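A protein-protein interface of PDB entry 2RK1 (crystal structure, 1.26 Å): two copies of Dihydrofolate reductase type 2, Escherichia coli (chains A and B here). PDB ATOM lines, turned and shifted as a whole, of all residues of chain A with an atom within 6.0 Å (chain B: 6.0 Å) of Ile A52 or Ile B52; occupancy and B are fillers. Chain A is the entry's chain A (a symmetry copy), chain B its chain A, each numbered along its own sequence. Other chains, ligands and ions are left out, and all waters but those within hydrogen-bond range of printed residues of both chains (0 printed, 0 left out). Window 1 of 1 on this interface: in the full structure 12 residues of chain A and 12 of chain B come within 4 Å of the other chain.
Among the printed residues, pairs that only touch across the chains: Tyr A30 with Ala B40, Ala A40 with Tyr B30, Val A50 with Ile B52, Ile A52 with Val B50 and Ile A52 with Ile B52.
Of the 9 printed residues of chain B, 4 touch a printed residue of chain A.
Printed residues of chain B that touch a printed residue of chain A: Tyr B30, Ala B40, Val B50 and Ile B52.
Hydrophobic or aromatic side chains of chain B that line the printed part of chain A: Tyr B30, Ala B40, Val B50 and Ile B52.
Among the printed residues, no Asp or Glu carboxylate lies within 4 Å of a Lys or Arg side-chain nitrogen of the other chain.
Tyr A30 touches Ala B40, and with the chains exchanged Ala A40 touches Tyr B30.
Val A50 touches Ile B52, and with the chains exchanged Ile A52 touches Val B50.
Ile B52 touches its own counterpart, Ile A52.
Positions printed for both chains: 30, 39, 40, 41, 50, 51, 52, 53 and 54.
Printed residues of chain B within 4 Å of Ala A40: Tyr B30 (3.9 Å).
Of the printed residues of chain B, Ile A52 touches Val B50 and Ile B52.
Tyr A53 touches none of the printed residues of chain B.
Of the printed residues of chain A, Tyr B30 touches Ala A40.
Of chain A, only Val A50 and Ile A52 come within 4 Å of Ile B52.
The nearest printed residue of chain A that does not touch Ile B52 is Gln A51 (4.8 Å).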
ATOM      1  N   TYR A  30       5.361   8.198  14.174  1.00  0.00           N
ATOM      2  CA  TYR A  30       6.644   7.548  14.227  1.00  0.00           C
ATOM      3  C   TYR A  30       7.007   7.025  12.856  1.00  0.00           C
ATOM      4  O   TYR A  30       6.144   6.889  11.974  1.00  0.00           O
ATOM      5  CB  TYR A  30       6.674   6.418  15.270  1.00  0.00           C
ATOM      6  CG  TYR A  30       5.883   5.187  14.954  1.00  0.00           C
ATOM      7  CD1 TYR A  30       4.497   5.232  15.068  1.00  0.00           C
ATOM      8  CD2 TYR A  30       6.454   4.004  14.525  1.00  0.00           C
ATOM      9  CE1 TYR A  30       3.708   4.164  14.752  1.00  0.00           C
ATOM     10  CE2 TYR A  30       5.695   2.908  14.249  1.00  0.00           C
ATOM     11  CZ  TYR A  30       4.304   2.967  14.348  1.00  0.00           C
ATOM     12  OH  TYR A  30       3.519   1.873  14.091  1.00  0.00           O
ATOM     13  N   TYR A  39       1.410   6.185  13.192  1.00  0.00           N
ATOM     14  CA  TYR A  39       0.693   7.098  14.031  1.00  0.00           C
ATOM     15  C   TYR A  39       0.439   6.532  15.408  1.00  0.00           C
ATOM     16  O   TYR A  39       0.201   5.351  15.576  1.00  0.00           O
ATOM     17  CB  TYR A  39      -0.649   7.494  13.383  1.00  0.00           C
ATOM     18  CG  TYR A  39      -0.454   8.284  12.103  1.00  0.00           C
ATOM     19  CD1 TYR A  39      -0.216   9.621  12.153  1.00  0.00           C
ATOM     20  CD2 TYR A  39      -0.408   7.677  10.870  1.00  0.00           C
ATOM     21  CE1 TYR A  39       0.034  10.350  11.015  1.00  0.00           C
ATOM     22  CE2 TYR A  39      -0.171   8.404   9.710  1.00  0.00           C
ATOM     23  CZ  TYR A  39       0.049   9.731   9.800  1.00  0.00           C
ATOM     24  OH  TYR A  39       0.313  10.510   8.670  1.00  0.00           O
ATOM     25  N   ALA A  40       0.447   7.427  16.360  1.00  0.00           N
ATOM     26  CA  ALA A  40      -0.025   7.166  17.728  1.00  0.00           C
ATOM     27  C   ALA A  40      -1.458   7.656  17.850  1.00  0.00           C
ATOM     28  O   ALA A  40      -1.759   8.781  17.450  1.00  0.00           O
ATOM     29  CB  ALA A  40       0.864   7.870  18.734  1.00  0.00           C
ATOM     30  N   VAL A  41      -2.329   6.805  18.404  1.00  0.00           N
ATOM     31  CA  VAL A  41      -3.734   7.069  18.530  1.00  0.00           C
ATOM     32  C   VAL A  41      -4.166   6.892  19.965  1.00  0.00           C
ATOM     33  O   VAL A  41      -4.007   5.798  20.522  1.00  0.00           O
ATOM     34  CB  VAL A  41      -4.548   6.151  17.613  1.00  0.00           C
ATOM     35  CG1 VAL A  41      -6.046   6.512  17.677  1.00  0.00           C
ATOM     36  CG2 VAL A  41      -4.072   6.190  16.180  1.00  0.00           C
ATOM     37  N   VAL A  50      -2.743   4.797  24.624  1.00  0.00           N
ATOM     38  CA  VAL A  50      -2.262   5.098  23.297  1.00  0.00           C
ATOM     39  C   VAL A  50      -1.713   3.823  22.686  1.00  0.00           C
ATOM     40  O   VAL A  50      -0.992   3.069  23.353  1.00  0.00           O
ATOM     41  CB  VAL A  50      -1.160   6.180  23.349  1.00  0.00           C
ATOM     42  CG1 VAL A  50      -0.624   6.507  21.955  1.00  0.00           C
ATOM     43  CG2 VAL A  50      -1.691   7.444  23.990  1.00  0.00           C
ATOM     44  N   GLN A  51      -2.051   3.617  21.410  1.00  0.00           N
ATOM     45  CA  GLN A  51      -1.484   2.535  20.635  1.00  0.00           C
ATOM     46  C   GLN A  51      -0.999   3.085  19.310  1.00  0.00           C
ATOM     47  O   GLN A  51      -1.552   4.045  18.786  1.00  0.00           O
ATOM     48  CB  GLN A  51      -2.492   1.411  20.382  1.00  0.00           C
ATOM     49  CG  GLN A  51      -2.606   0.534  21.624  1.00  0.00           C
ATOM     50  CD  GLN A  51      -3.365  -0.755  21.428  1.00  0.00           C
ATOM     51  OE1 GLN A  51      -3.891  -1.025  20.346  1.00  0.00           O
ATOM     52  NE2 GLN A  51      -3.448  -1.552  22.488  1.00  0.00           N
ATOM     53  N   ILE A  52       0.042   2.449  18.768  1.00  0.00           N
ATOM     54  CA  ILE A  52       0.698   2.892  17.545  1.00  0.00           C
ATOM     55  C   ILE A  52       0.443   1.902  16.411  1.00  0.00           C
ATOM     56  O   ILE A  52       0.482   0.688  16.611  1.00  0.00           O
ATOM     57  CB  ILE A  52       2.216   3.098  17.754  1.00  0.00           C
ATOM     58  CG1 ILE A  52       2.899   1.869  18.340  1.00  0.00           C
ATOM     59  CG2 ILE A  52       2.470   4.325  18.593  1.00  0.00           C
ATOM     60  CD1 ILE A  52       4.455   1.952  18.259  1.00  0.00           C
ATOM     61  N   TYR A  53       0.233   2.454  15.239  1.00  0.00           N
ATOM     62  CA  TYR A  53      -0.088   1.657  14.058  1.00  0.00           C
ATOM     63  C   TYR A  53       0.459   2.264  12.777  1.00  0.00           C
ATOM     64  O   TYR A  53       0.515   3.491  12.609  1.00  0.00           O
ATOM     65  CB  TYR A  53      -1.592   1.558  13.834  1.00  0.00           C
ATOM     66  CG  TYR A  53      -2.371   0.996  15.008  1.00  0.00           C
ATOM     67  CD1 TYR A  53      -2.425  -0.370  15.248  1.00  0.00           C
ATOM     68  CD2 TYR A  53      -3.030   1.819  15.902  1.00  0.00           C
ATOM     69  CE1 TYR A  53      -3.131  -0.858  16.378  1.00  0.00           C
ATOM     70  CE2 TYR A  53      -3.731   1.302  16.971  1.00  0.00           C
ATOM     71  CZ  TYR A  53      -3.792   0.017  17.192  1.00  0.00           C
ATOM     72  OH  TYR A  53      -4.572  -0.341  18.297  1.00  0.00           O
ATOM     73  N   PRO A  54       0.755   1.406  11.794  1.00  0.00           N
ATOM     74  CA  PRO A  54       1.067   1.922  10.462  1.00  0.00           C
ATOM     75  C   PRO A  54      -0.128   2.635   9.855  1.00  0.00           C
ATOM     76  O   PRO A  54      -1.278   2.257  10.092  1.00  0.00           O
ATOM     77  CB  PRO A  54       1.429   0.661   9.664  1.00  0.00           C
ATOM     78  CG  PRO A  54       1.736  -0.367  10.670  1.00  0.00           C
ATOM     79  CD  PRO A  54       0.818  -0.050  11.841  1.00  0.00           C
ATOM     80  N   TYR B  30       4.750  11.558  20.798  1.00  0.00           N
ATOM     81  CA  TYR B  30       3.331  11.683  20.999  1.00  0.00           C
ATOM     82  C   TYR B  30       3.061  12.566  22.196  1.00  0.00           C
ATOM     83  O   TYR B  30       3.950  12.802  23.029  1.00  0.00           O
ATOM     84  CB  TYR B  30       2.650  10.314  21.165  1.00  0.00           C
ATOM     85  CG  TYR B  30       2.929   9.572  22.434  1.00  0.00           C
ATOM     86  CD1 TYR B  30       4.166   8.957  22.595  1.00  0.00           C
ATOM     87  CD2 TYR B  30       2.027   9.483  23.478  1.00  0.00           C
ATOM     88  CE1 TYR B  30       4.508   8.302  23.744  1.00  0.00           C
ATOM     89  CE2 TYR B  30       2.322   8.795  24.616  1.00  0.00           C
ATOM     90  CZ  TYR B  30       3.573   8.198  24.777  1.00  0.00           C
ATOM     91  OH  TYR B  30       3.889   7.488  25.906  1.00  0.00           O
ATOM     92  N   TYR B  39       7.676   9.628  23.687  1.00  0.00           N
ATOM     93  CA  TYR B  39       8.521   9.209  22.608  1.00  0.00           C
ATOM     94  C   TYR B  39       8.257   7.781  22.196  1.00  0.00           C
ATOM     95  O   TYR B  39       7.966   6.926  23.012  1.00  0.00           O
ATOM     96  CB  TYR B  39      10.007   9.367  22.989  1.00  0.00           C
ATOM     97  CG  TYR B  39      10.395  10.820  23.184  1.00  0.00           C
ATOM     98  CD1 TYR B  39      10.706  11.596  22.113  1.00  0.00           C
ATOM     99  CD2 TYR B  39      10.350  11.428  24.417  1.00  0.00           C
ATOM    100  CE1 TYR B  39      10.994  12.932  22.253  1.00  0.00           C
ATOM    101  CE2 TYR B  39      10.652  12.775  24.574  1.00  0.00           C
ATOM    102  CZ  TYR B  39      10.968  13.509  23.489  1.00  0.00           C
ATOM    103  OH  TYR B  39      11.260  14.873  23.583  1.00  0.00           O
ATOM    104  N   ALA B  40       8.423   7.557  20.919  1.00  0.00           N
ATOM    105  CA  ALA B  40       8.478   6.212  20.328  1.00  0.00           C
ATOM    106  C   ALA B  40       9.935   5.812  20.162  1.00  0.00           C
ATOM    107  O   ALA B  40      10.731   6.593  19.641  1.00  0.00           O
ATOM    108  CB  ALA B  40       7.769   6.198  18.988  1.00  0.00           C
ATOM    109  N   VAL B  41      10.268   4.595  20.608  1.00  0.00           N
ATOM    110  CA  VAL B  41      11.608   4.082  20.602  1.00  0.00           C
ATOM    111  C   VAL B  41      11.647   2.748  19.897  1.00  0.00           C
ATOM    112  O   VAL B  41      10.960   1.811  20.322  1.00  0.00           O
ATOM    113  CB  VAL B  41      12.148   3.945  22.029  1.00  0.00           C
ATOM    114  CG1 VAL B  41      13.622   3.492  22.009  1.00  0.00           C
ATOM    115  CG2 VAL B  41      12.014   5.221  22.826  1.00  0.00           C
ATOM    116  N   VAL B  50       8.635  -1.270  18.193  1.00  0.00           N
ATOM    117  CA  VAL B  50       8.580   0.071  18.727  1.00  0.00           C
ATOM    118  C   VAL B  50       7.697   0.059  19.960  1.00  0.00           C
ATOM    119  O   VAL B  50       6.621  -0.553  19.953  1.00  0.00           O
ATOM    120  CB  VAL B  50       8.015   1.053  17.677  1.00  0.00           C
ATOM    121  CG1 VAL B  50       7.935   2.478  18.224  1.00  0.00           C
ATOM    122  CG2 VAL B  50       8.872   1.043  16.429  1.00  0.00           C
ATOM    123  N   GLN B  51       8.164   0.761  20.996  1.00  0.00           N
ATOM    124  CA  GLN B  51       7.374   0.982  22.187  1.00  0.00           C
ATOM    125  C   GLN B  51       7.414   2.455  22.533  1.00  0.00           C
ATOM    126  O   GLN B  51       8.395   3.140  22.263  1.00  0.00           O
ATOM    127  CB  GLN B  51       7.876   0.164  23.379  1.00  0.00           C
ATOM    128  CG  GLN B  51       7.388  -1.275  23.257  1.00  0.00           C
ATOM    129  CD  GLN B  51       7.591  -2.125  24.487  1.00  0.00           C
ATOM    130  OE1 GLN B  51       8.164  -1.677  25.482  1.00  0.00           O
ATOM    131  NE2 GLN B  51       7.142  -3.374  24.415  1.00  0.00           N
ATOM    132  N   ILE B  52       6.333   2.933  23.152  1.00  0.00           N
ATOM    133  CA  ILE B  52       6.157   4.342  23.480  1.00  0.00           C
ATOM    134  C   ILE B  52       6.210   4.551  24.993  1.00  0.00           C
ATOM    135  O   ILE B  52       5.651   3.766  25.759  1.00  0.00           O
ATOM    136  CB  ILE B  52       4.840   4.904  22.900  1.00  0.00           C
ATOM    137  CG1 ILE B  52       3.623   4.082  23.306  1.00  0.00           C
ATOM    138  CG2 ILE B  52       4.940   5.041  21.402  1.00  0.00           C
ATOM    139  CD1 ILE B  52       2.277   4.807  22.996  1.00  0.00           C
ATOM    140  N   TYR B  53       6.844   5.634  25.374  1.00  0.00           N
ATOM    141  CA  TYR B  53       7.042   5.955  26.784  1.00  0.00           C
ATOM    142  C   TYR B  53       7.042   7.451  27.049  1.00  0.00           C
ATOM    143  O   TYR B  53       7.514   8.257  26.234  1.00  0.00           O
ATOM    144  CB  TYR B  53       8.394   5.467  27.292  1.00  0.00           C
ATOM    145  CG  TYR B  53       8.640   3.982  27.108  1.00  0.00           C
ATOM    146  CD1 TYR B  53       8.096   3.049  27.979  1.00  0.00           C
ATOM    147  CD2 TYR B  53       9.387   3.497  26.050  1.00  0.00           C
ATOM    148  CE1 TYR B  53       8.316   1.665  27.754  1.00  0.00           C
ATOM    149  CE2 TYR B  53       9.602   2.145  25.885  1.00  0.00           C
ATOM    150  CZ  TYR B  53       9.101   1.266  26.710  1.00  0.00           C
ATOM    151  OH  TYR B  53       9.443  -0.059  26.418  1.00  0.00           O
ATOM    152  N   PRO B  54       6.623   7.839  28.259  1.00  0.00           N
ATOM    153  CA  PRO B  54       6.807   9.231  28.670  1.00  0.00           C
ATOM    154  C   PRO B  54       8.281   9.587  28.759  1.00  0.00           C
ATOM    155  O   PRO B  54       9.114   8.748  29.110  1.00  0.00           O
ATOM    156  CB  PRO B  54       6.133   9.291  30.047  1.00  0.00           C
ATOM    157  CG  PRO B  54       5.253   8.115  30.107  1.00  0.00           C
ATOM    158  CD  PRO B  54       5.976   7.048  29.299  1.00  0.00           C
